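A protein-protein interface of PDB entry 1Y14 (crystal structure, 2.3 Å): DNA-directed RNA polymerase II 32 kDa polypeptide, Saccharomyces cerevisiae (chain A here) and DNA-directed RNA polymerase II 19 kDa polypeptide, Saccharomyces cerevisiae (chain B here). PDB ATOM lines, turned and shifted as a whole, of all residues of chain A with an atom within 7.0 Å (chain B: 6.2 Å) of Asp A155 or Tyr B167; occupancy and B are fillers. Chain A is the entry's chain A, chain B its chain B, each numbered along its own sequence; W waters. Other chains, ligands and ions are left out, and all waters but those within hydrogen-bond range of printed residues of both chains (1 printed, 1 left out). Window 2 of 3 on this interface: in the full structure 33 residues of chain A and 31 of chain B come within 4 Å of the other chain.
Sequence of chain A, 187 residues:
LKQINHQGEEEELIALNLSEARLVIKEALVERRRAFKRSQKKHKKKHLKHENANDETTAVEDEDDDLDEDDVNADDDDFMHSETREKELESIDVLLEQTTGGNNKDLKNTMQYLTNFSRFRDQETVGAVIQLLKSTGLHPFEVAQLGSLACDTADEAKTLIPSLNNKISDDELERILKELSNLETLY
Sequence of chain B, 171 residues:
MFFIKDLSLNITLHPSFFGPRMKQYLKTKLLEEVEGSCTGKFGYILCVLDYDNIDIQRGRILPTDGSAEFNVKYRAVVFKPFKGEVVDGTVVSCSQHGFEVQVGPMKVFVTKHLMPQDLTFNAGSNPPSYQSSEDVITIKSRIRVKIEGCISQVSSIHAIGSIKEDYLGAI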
ATOM      1  N   ASP A 152      13.494 -34.203 -29.143  1.00  0.00           N
ATOM      2  CA  ASP A 152      12.536 -34.953 -28.337  1.00  0.00           C
ATOM      3  C   ASP A 152      11.252 -34.209 -28.002  1.00  0.00           C
ATOM      4  O   ASP A 152      10.200 -34.835 -27.872  1.00  0.00           O
ATOM      5  CB  ASP A 152      13.195 -35.436 -27.042  1.00  0.00           C
ATOM      6  CG  ASP A 152      14.366 -36.365 -27.305  1.00  0.00           C
ATOM      7  OD1 ASP A 152      14.203 -37.308 -28.115  1.00  0.00           O
ATOM      8  OD2 ASP A 152      15.445 -36.154 -26.705  1.00  0.00           O
ATOM      9  N   THR A 153      11.321 -32.887 -27.866  1.00  0.00           N
ATOM     10  CA  THR A 153      10.119 -32.117 -27.528  1.00  0.00           C
ATOM     11  C   THR A 153       9.856 -30.921 -28.437  1.00  0.00           C
ATOM     12  O   THR A 153      10.757 -30.419 -29.105  1.00  0.00           O
ATOM     13  CB  THR A 153      10.186 -31.600 -26.083  1.00  0.00           C
ATOM     14  OG1 THR A 153      11.277 -30.676 -25.949  1.00  0.00           O
ATOM     15  CG2 THR A 153      10.393 -32.756 -25.118  1.00  0.00           C
ATOM     16  N   ALA A 154       8.607 -30.470 -28.451  1.00  0.00           N
ATOM     17  CA  ALA A 154       8.203 -29.324 -29.253  1.00  0.00           C
ATOM     18  C   ALA A 154       9.040 -28.097 -28.889  1.00  0.00           C
ATOM     19  O   ALA A 154       9.497 -27.355 -29.767  1.00  0.00           O
ATOM     20  CB  ALA A 154       6.727 -29.037 -29.031  1.00  0.00           C
ATOM     21  N   ASP A 155       9.250 -27.890 -27.593  1.00  0.00           N
ATOM     22  CA  ASP A 155      10.040 -26.753 -27.128  1.00  0.00           C
ATOM     23  C   ASP A 155      11.476 -26.824 -27.641  1.00  0.00           C
ATOM     24  O   ASP A 155      12.065 -25.804 -27.997  1.00  0.00           O
ATOM     25  CB  ASP A 155      10.065 -26.692 -25.601  1.00  0.00           C
ATOM     26  CG  ASP A 155      10.816 -25.476 -25.084  1.00  0.00           C
ATOM     27  OD1 ASP A 155      10.370 -24.341 -25.361  1.00  0.00           O
ATOM     28  OD2 ASP A 155      11.856 -25.653 -24.409  1.00  0.00           O
ATOM     29  N   GLU A 156      12.043 -28.025 -27.669  1.00  0.00           N
ATOM     30  CA  GLU A 156      13.408 -28.191 -28.160  1.00  0.00           C
ATOM     31  C   GLU A 156      13.485 -27.782 -29.639  1.00  0.00           C
ATOM     32  O   GLU A 156      14.314 -26.954 -30.026  1.00  0.00           O
ATOM     33  CB  GLU A 156      13.870 -29.645 -28.004  1.00  0.00           C
ATOM     34  CG  GLU A 156      15.278 -29.868 -28.535  1.00  0.00           C
ATOM     35  CD  GLU A 156      15.794 -31.276 -28.293  1.00  0.00           C
ATOM     36  OE1 GLU A 156      17.010 -31.493 -28.474  1.00  0.00           O
ATOM     37  OE2 GLU A 156      14.992 -32.165 -27.932  1.00  0.00           O
ATOM     38  N   ALA A 157      12.613 -28.364 -30.454  1.00  0.00           N
ATOM     39  CA  ALA A 157      12.576 -28.058 -31.882  1.00  0.00           C
ATOM     40  C   ALA A 157      12.278 -26.577 -32.135  1.00  0.00           C
ATOM     41  O   ALA A 157      12.964 -25.927 -32.922  1.00  0.00           O
ATOM     42  CB  ALA A 157      11.537 -28.925 -32.562  1.00  0.00           C
ATOM     43  N   LYS A 158      11.258 -26.038 -31.474  1.00  0.00           N
ATOM     44  CA  LYS A 158      10.925 -24.626 -31.666  1.00  0.00           C
ATOM     45  C   LYS A 158      12.040 -23.727 -31.186  1.00  0.00           C
ATOM     46  O   LYS A 158      12.229 -22.633 -31.713  1.00  0.00           O
ATOM     47  CB  LYS A 158       9.614 -24.264 -30.966  1.00  0.00           C
ATOM     48  CG  LYS A 158       8.392 -24.812 -31.689  1.00  0.00           C
ATOM     49  CD  LYS A 158       7.076 -24.276 -31.114  1.00  0.00           C
ATOM     50  CE  LYS A 158       5.901 -24.695 -31.993  1.00  0.00           C
ATOM     51  NZ  LYS A 158       4.590 -24.192 -31.501  1.00  0.00           N
ATOM     52  N   THR A 159      12.803 -24.186 -30.202  1.00  0.00           N
ATOM     53  CA  THR A 159      13.923 -23.382 -29.721  1.00  0.00           C
ATOM     54  C   THR A 159      15.070 -23.421 -30.739  1.00  0.00           C
ATOM     55  O   THR A 159      15.699 -22.399 -31.009  1.00  0.00           O
ATOM     56  CB  THR A 159      14.458 -23.889 -28.384  1.00  0.00           C
ATOM     57  OG1 THR A 159      13.404 -23.893 -27.417  1.00  0.00           O
ATOM     58  CG2 THR A 159      15.592 -22.983 -27.901  1.00  0.00           C
ATOM     59  N   LEU A 160      15.324 -24.601 -31.311  1.00  0.00           N
ATOM     60  CA  LEU A 160      16.396 -24.771 -32.293  1.00  0.00           C
ATOM     61  C   LEU A 160      16.024 -24.262 -33.685  1.00  0.00           C
ATOM     62  O   LEU A 160      16.894 -23.839 -34.441  1.00  0.00           O
ATOM     63  CB  LEU A 160      16.816 -26.245 -32.375  1.00  0.00           C
ATOM     64  CG  LEU A 160      17.283 -26.913 -31.069  1.00  0.00           C
ATOM     65  CD1 LEU A 160      17.834 -28.296 -31.388  1.00  0.00           C
ATOM     66  CD2 LEU A 160      18.365 -26.063 -30.376  1.00  0.00           C
ATOM     67  N   ILE A 161      14.739 -24.314 -34.028  1.00  0.00           N
ATOM     68  CA  ILE A 161      14.268 -23.829 -35.327  1.00  0.00           C
ATOM     69  C   ILE A 161      13.152 -22.827 -34.995  1.00  0.00           C
ATOM     70  O   ILE A 161      11.968 -23.085 -35.236  1.00  0.00           O
ATOM     71  CB  ILE A 161      13.690 -24.976 -36.180  1.00  0.00           C
ATOM     72  CG1 ILE A 161      14.655 -26.149 -36.178  1.00  0.00           C
ATOM     73  CG2 ILE A 161      13.452 -24.502 -37.635  1.00  0.00           C
ATOM     74  CD1 ILE A 161      14.114 -27.374 -36.910  1.00  0.00           C
ATOM     75  N   ASN A 165       7.918 -21.456 -34.360  1.00  0.00           N
ATOM     76  CA  ASN A 165       7.112 -20.850 -33.297  1.00  0.00           C
ATOM     77  C   ASN A 165       5.650 -20.550 -33.614  1.00  0.00           C
ATOM     78  O   ASN A 165       4.750 -21.024 -32.914  1.00  0.00           O
ATOM     79  CB  ASN A 165       7.784 -19.560 -32.813  1.00  0.00           C
ATOM     80  CG  ASN A 165       8.711 -19.788 -31.633  1.00  0.00           C
ATOM     81  OD1 ASN A 165       9.565 -18.948 -31.329  1.00  0.00           O
ATOM     82  ND2 ASN A 165       8.541 -20.917 -30.950  1.00  0.00           N
ATOM     83  N   ASP A 170       2.433 -26.834 -30.688  1.00  0.00           N
ATOM     84  CA  ASP A 170       3.254 -27.796 -29.969  1.00  0.00           C
ATOM     85  C   ASP A 170       2.673 -29.185 -30.167  1.00  0.00           C
ATOM     86  O   ASP A 170       3.385 -30.156 -30.395  1.00  0.00           O
ATOM     87  CB  ASP A 170       3.270 -27.469 -28.480  1.00  0.00           C
ATOM     88  CG  ASP A 170       4.076 -26.236 -28.176  1.00  0.00           C
ATOM     89  OD1 ASP A 170       4.325 -25.967 -26.984  1.00  0.00           O
ATOM     90  OD2 ASP A 170       4.460 -25.535 -29.134  1.00  0.00           O
ATOM     91  N   LEU A 173       3.361 -30.585 -33.663  1.00  0.00           N
ATOM     92  CA  LEU A 173       4.782 -30.811 -33.874  1.00  0.00           C
ATOM     93  C   LEU A 173       5.245 -32.019 -33.062  1.00  0.00           C
ATOM     94  O   LEU A 173       6.185 -32.712 -33.447  1.00  0.00           O
ATOM     95  CB  LEU A 173       5.574 -29.569 -33.466  1.00  0.00           C
ATOM     96  CG  LEU A 173       7.098 -29.637 -33.571  1.00  0.00           C
ATOM     97  CD1 LEU A 173       7.497 -29.992 -34.998  1.00  0.00           C
ATOM     98  CD2 LEU A 173       7.695 -28.295 -33.159  1.00  0.00           C
ATOM     99  N   GLU A 174       4.584 -32.261 -31.934  1.00  0.00           N
ATOM    100  CA  GLU A 174       4.923 -33.392 -31.079  1.00  0.00           C
ATOM    101  C   GLU A 174       4.650 -34.698 -31.820  1.00  0.00           C
ATOM    102  O   GLU A 174       5.414 -35.658 -31.704  1.00  0.00           O
ATOM    103  CB  GLU A 174       4.098 -33.351 -29.789  1.00  0.00           C
ATOM    104  CG  GLU A 174       4.547 -32.297 -28.784  1.00  0.00           C
ATOM    105  CD  GLU A 174       5.774 -32.717 -27.993  1.00  0.00           C
ATOM    106  OE1 GLU A 174       6.359 -31.860 -27.293  1.00  0.00           O
ATOM    107  OE2 GLU A 174       6.149 -33.909 -28.060  1.00  0.00           O
ATOM    108  N   LEU A 177       7.288 -35.297 -34.415  1.00  0.00           N
ATOM    109  CA  LEU A 177       8.484 -35.730 -33.705  1.00  0.00           C
ATOM    110  C   LEU A 177       8.421 -37.220 -33.348  1.00  0.00           C
ATOM    111  O   LEU A 177       9.402 -37.948 -33.516  1.00  0.00           O
ATOM    112  CB  LEU A 177       8.664 -34.886 -32.438  1.00  0.00           C
ATOM    113  CG  LEU A 177       9.567 -33.651 -32.555  1.00  0.00           C
ATOM    114  CD1 LEU A 177       9.292 -32.918 -33.846  1.00  0.00           C
ATOM    115  CD2 LEU A 177       9.352 -32.744 -31.362  1.00  0.00           C
ATOM    116  N   VAL B  86      21.334 -24.494 -36.827  1.00  0.00           N
ATOM    117  CA  VAL B  86      21.818 -25.376 -35.769  1.00  0.00           C
ATOM    118  C   VAL B  86      22.238 -26.683 -36.448  1.00  0.00           C
ATOM    119  O   VAL B  86      21.487 -27.244 -37.246  1.00  0.00           O
ATOM    120  CB  VAL B  86      20.730 -25.659 -34.732  1.00  0.00           C
ATOM    121  CG1 VAL B  86      21.194 -26.774 -33.760  1.00  0.00           C
ATOM    122  CG2 VAL B  86      20.413 -24.375 -33.964  1.00  0.00           C
ATOM    123  N   ARG B 144      26.016 -30.417 -30.559  1.00  0.00           N
ATOM    124  CA  ARG B 144      25.061 -29.589 -31.287  1.00  0.00           C
ATOM    125  C   ARG B 144      25.489 -28.129 -31.159  1.00  0.00           C
ATOM    126  O   ARG B 144      25.603 -27.588 -30.057  1.00  0.00           O
ATOM    127  CB  ARG B 144      23.658 -29.786 -30.716  1.00  0.00           C
ATOM    128  CG  ARG B 144      22.595 -28.963 -31.413  1.00  0.00           C
ATOM    129  CD  ARG B 144      21.251 -29.636 -31.298  1.00  0.00           C
ATOM    130  NE  ARG B 144      21.206 -30.881 -32.060  1.00  0.00           N
ATOM    131  CZ  ARG B 144      20.199 -31.747 -32.010  1.00  0.00           C
ATOM    132  NH1 ARG B 144      19.153 -31.504 -31.228  1.00  0.00           N
ATOM    133  NH2 ARG B 144      20.234 -32.857 -32.738  1.00  0.00           N
ATOM    134  N   GLU B 165      23.234 -21.246 -25.723  1.00  0.00           N
ATOM    135  CA  GLU B 165      21.782 -21.357 -25.671  1.00  0.00           C
ATOM    136  C   GLU B 165      21.259 -22.719 -25.253  1.00  0.00           C
ATOM    137  O   GLU B 165      21.992 -23.705 -25.235  1.00  0.00           O
ATOM    138  CB  GLU B 165      21.183 -20.991 -27.032  1.00  0.00           C
ATOM    139  CG  GLU B 165      21.820 -19.780 -27.712  1.00  0.00           C
ATOM    140  CD  GLU B 165      21.824 -18.539 -26.840  1.00  0.00           C
ATOM    141  OE1 GLU B 165      20.757 -18.206 -26.275  1.00  0.00           O
ATOM    142  OE2 GLU B 165      22.892 -17.893 -26.728  1.00  0.00           O
ATOM    143  N   ASP B 166      19.968 -22.764 -24.942  1.00  0.00           N
ATOM    144  CA  ASP B 166      19.299 -23.995 -24.529  1.00  0.00           C
ATOM    145  C   ASP B 166      19.329 -25.049 -25.633  1.00  0.00           C
ATOM    146  O   ASP B 166      19.223 -24.729 -26.819  1.00  0.00           O
ATOM    147  CB  ASP B 166      17.828 -23.720 -24.164  1.00  0.00           C
ATOM    148  CG  ASP B 166      17.673 -22.743 -23.001  1.00  0.00           C
ATOM    149  OD1 ASP B 166      18.182 -23.027 -21.896  1.00  0.00           O
ATOM    150  OD2 ASP B 166      17.031 -21.690 -23.197  1.00  0.00           O
ATOM    151  N   TYR B 167      19.472 -26.307 -25.227  1.00  0.00           N
ATOM    152  CA  TYR B 167      19.494 -27.433 -26.152  1.00  0.00           C
ATOM    153  C   TYR B 167      20.723 -27.549 -27.064  1.00  0.00           C
ATOM    154  O   TYR B 167      20.731 -28.349 -27.993  1.00  0.00           O
ATOM    155  CB  TYR B 167      18.216 -27.422 -26.990  1.00  0.00           C
ATOM    156  CG  TYR B 167      16.953 -27.446 -26.153  1.00  0.00           C
ATOM    157  CD1 TYR B 167      16.100 -26.335 -26.102  1.00  0.00           C
ATOM    158  CD2 TYR B 167      16.606 -28.578 -25.414  1.00  0.00           C
ATOM    159  CE1 TYR B 167      14.932 -26.354 -25.337  1.00  0.00           C
ATOM    160  CE2 TYR B 167      15.440 -28.608 -24.641  1.00  0.00           C
ATOM    161  CZ  TYR B 167      14.612 -27.494 -24.610  1.00  0.00           C
ATOM    162  OH  TYR B 167      13.470 -27.524 -23.854  1.00  0.00           O
ATOM    163  N   LEU B 168      21.755 -26.753 -26.806  1.00  0.00           N
ATOM    164  CA  LEU B 168      22.978 -26.829 -27.598  1.00  0.00           C
ATOM    165  C   LEU B 168      24.046 -27.516 -26.755  1.00  0.00           C
ATOM    166  O   LEU B 168      23.920 -27.596 -25.538  1.00  0.00           O
ATOM    167  CB  LEU B 168      23.480 -25.442 -27.968  1.00  0.00           C
ATOM    168  CG  LEU B 168      22.556 -24.545 -28.777  1.00  0.00           C
ATOM    169  CD1 LEU B 168      23.340 -23.296 -29.172  1.00  0.00           C
ATOM    170  CD2 LEU B 168      22.059 -25.283 -30.014  1.00  0.00           C
ATOM    171  N   GLY B 169      25.095 -28.010 -27.398  1.00  0.00           N
ATOM    172  CA  GLY B 169      26.156 -28.668 -26.659  1.00  0.00           C
ATOM    173  C   GLY B 169      26.231 -30.181 -26.765  1.00  0.00           C
ATOM    174  O   GLY B 169      25.736 -30.788 -27.723  1.00  0.00           O
HETATM  175  O   HOH W   1      18.338 -23.717 -36.739  1.00  0.00           O
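OH of Tyr B167 sits at hydrogen-bond distance from OD2 of Asp A155.
NH1 of Arg B144 lies within salt-bridge range of OE1 of Glu A156.
The side-chain carboxylate (OE2) of Glu A156 lies within hydrogen-bond range of the backbone NH (N) of Asp A152, 2.8 Å away.
The side-chain hydroxyl (OG1) of Thr A153 lies within hydrogen-bond range of the backbone NH (N) of Glu A156, 3.3 Å away.
The backbone carbonyl oxygen of Asp A155 sits at hydrogen-bond distance from the side-chain hydroxyl of Thr A159 (2.4 Å).
O of Arg B144 lies within hydrogen-bond range of N of Gly B169, 2.7 Å away.
CG of Glu A156 touches CD2 of Tyr B167, 3.6 Å away.
Tyr B167 touches Thr A159.
Leu A160 touches Val B86.
Arg B144 touches Leu A160 (NH1 to CD1, 3.5 Å).
Leu A160 touches Asp B166.
Leu A160 touches Tyr B167 (CD2 to CB, 3.7 Å).
Leu A160 touches Leu B168.
Ala A157 touches none of the printed residues of chain B.
Of the printed residues of chain A, Val B86 touches Leu A160 (3.6 Å).
Printed residues of chain A within 4 Å of Arg B144: Glu A156 (3.5 Å) and Leu A160 (3.5 Å).
Of the printed residues of chain A, Tyr B167 touches Asp A155 (2.5 Å), Glu A156 (3.6 Å), Thr A159 (3.6 Å) and Leu A160 (3.7 Å).
The nearest residue of chain A that does not touch Tyr B167 is Thr A153 (4.4 Å).
Of the 15 printed residues of chain A, 4 touch a printed residue of chain B.
Hydrophobic or aromatic side chains of chain A that line the printed part of chain B: Leu A160.
Of the 7 printed residues of chain B, 5 touch a printed residue of chain A.
Hydrophobic or aromatic side chains of chain B that line the printed part of chain A: Val B86, Tyr B167 and Leu B168.
Along chain B the printed residues that touch a printed residue of chain A span positions 86 to 168.
Water W1 lies within hydrogen-bond range of the backbone carbonyl oxygen (O) of Leu A160 (2.7 Å) and the backbone NH (N) of Val B86 (3.1 Å).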
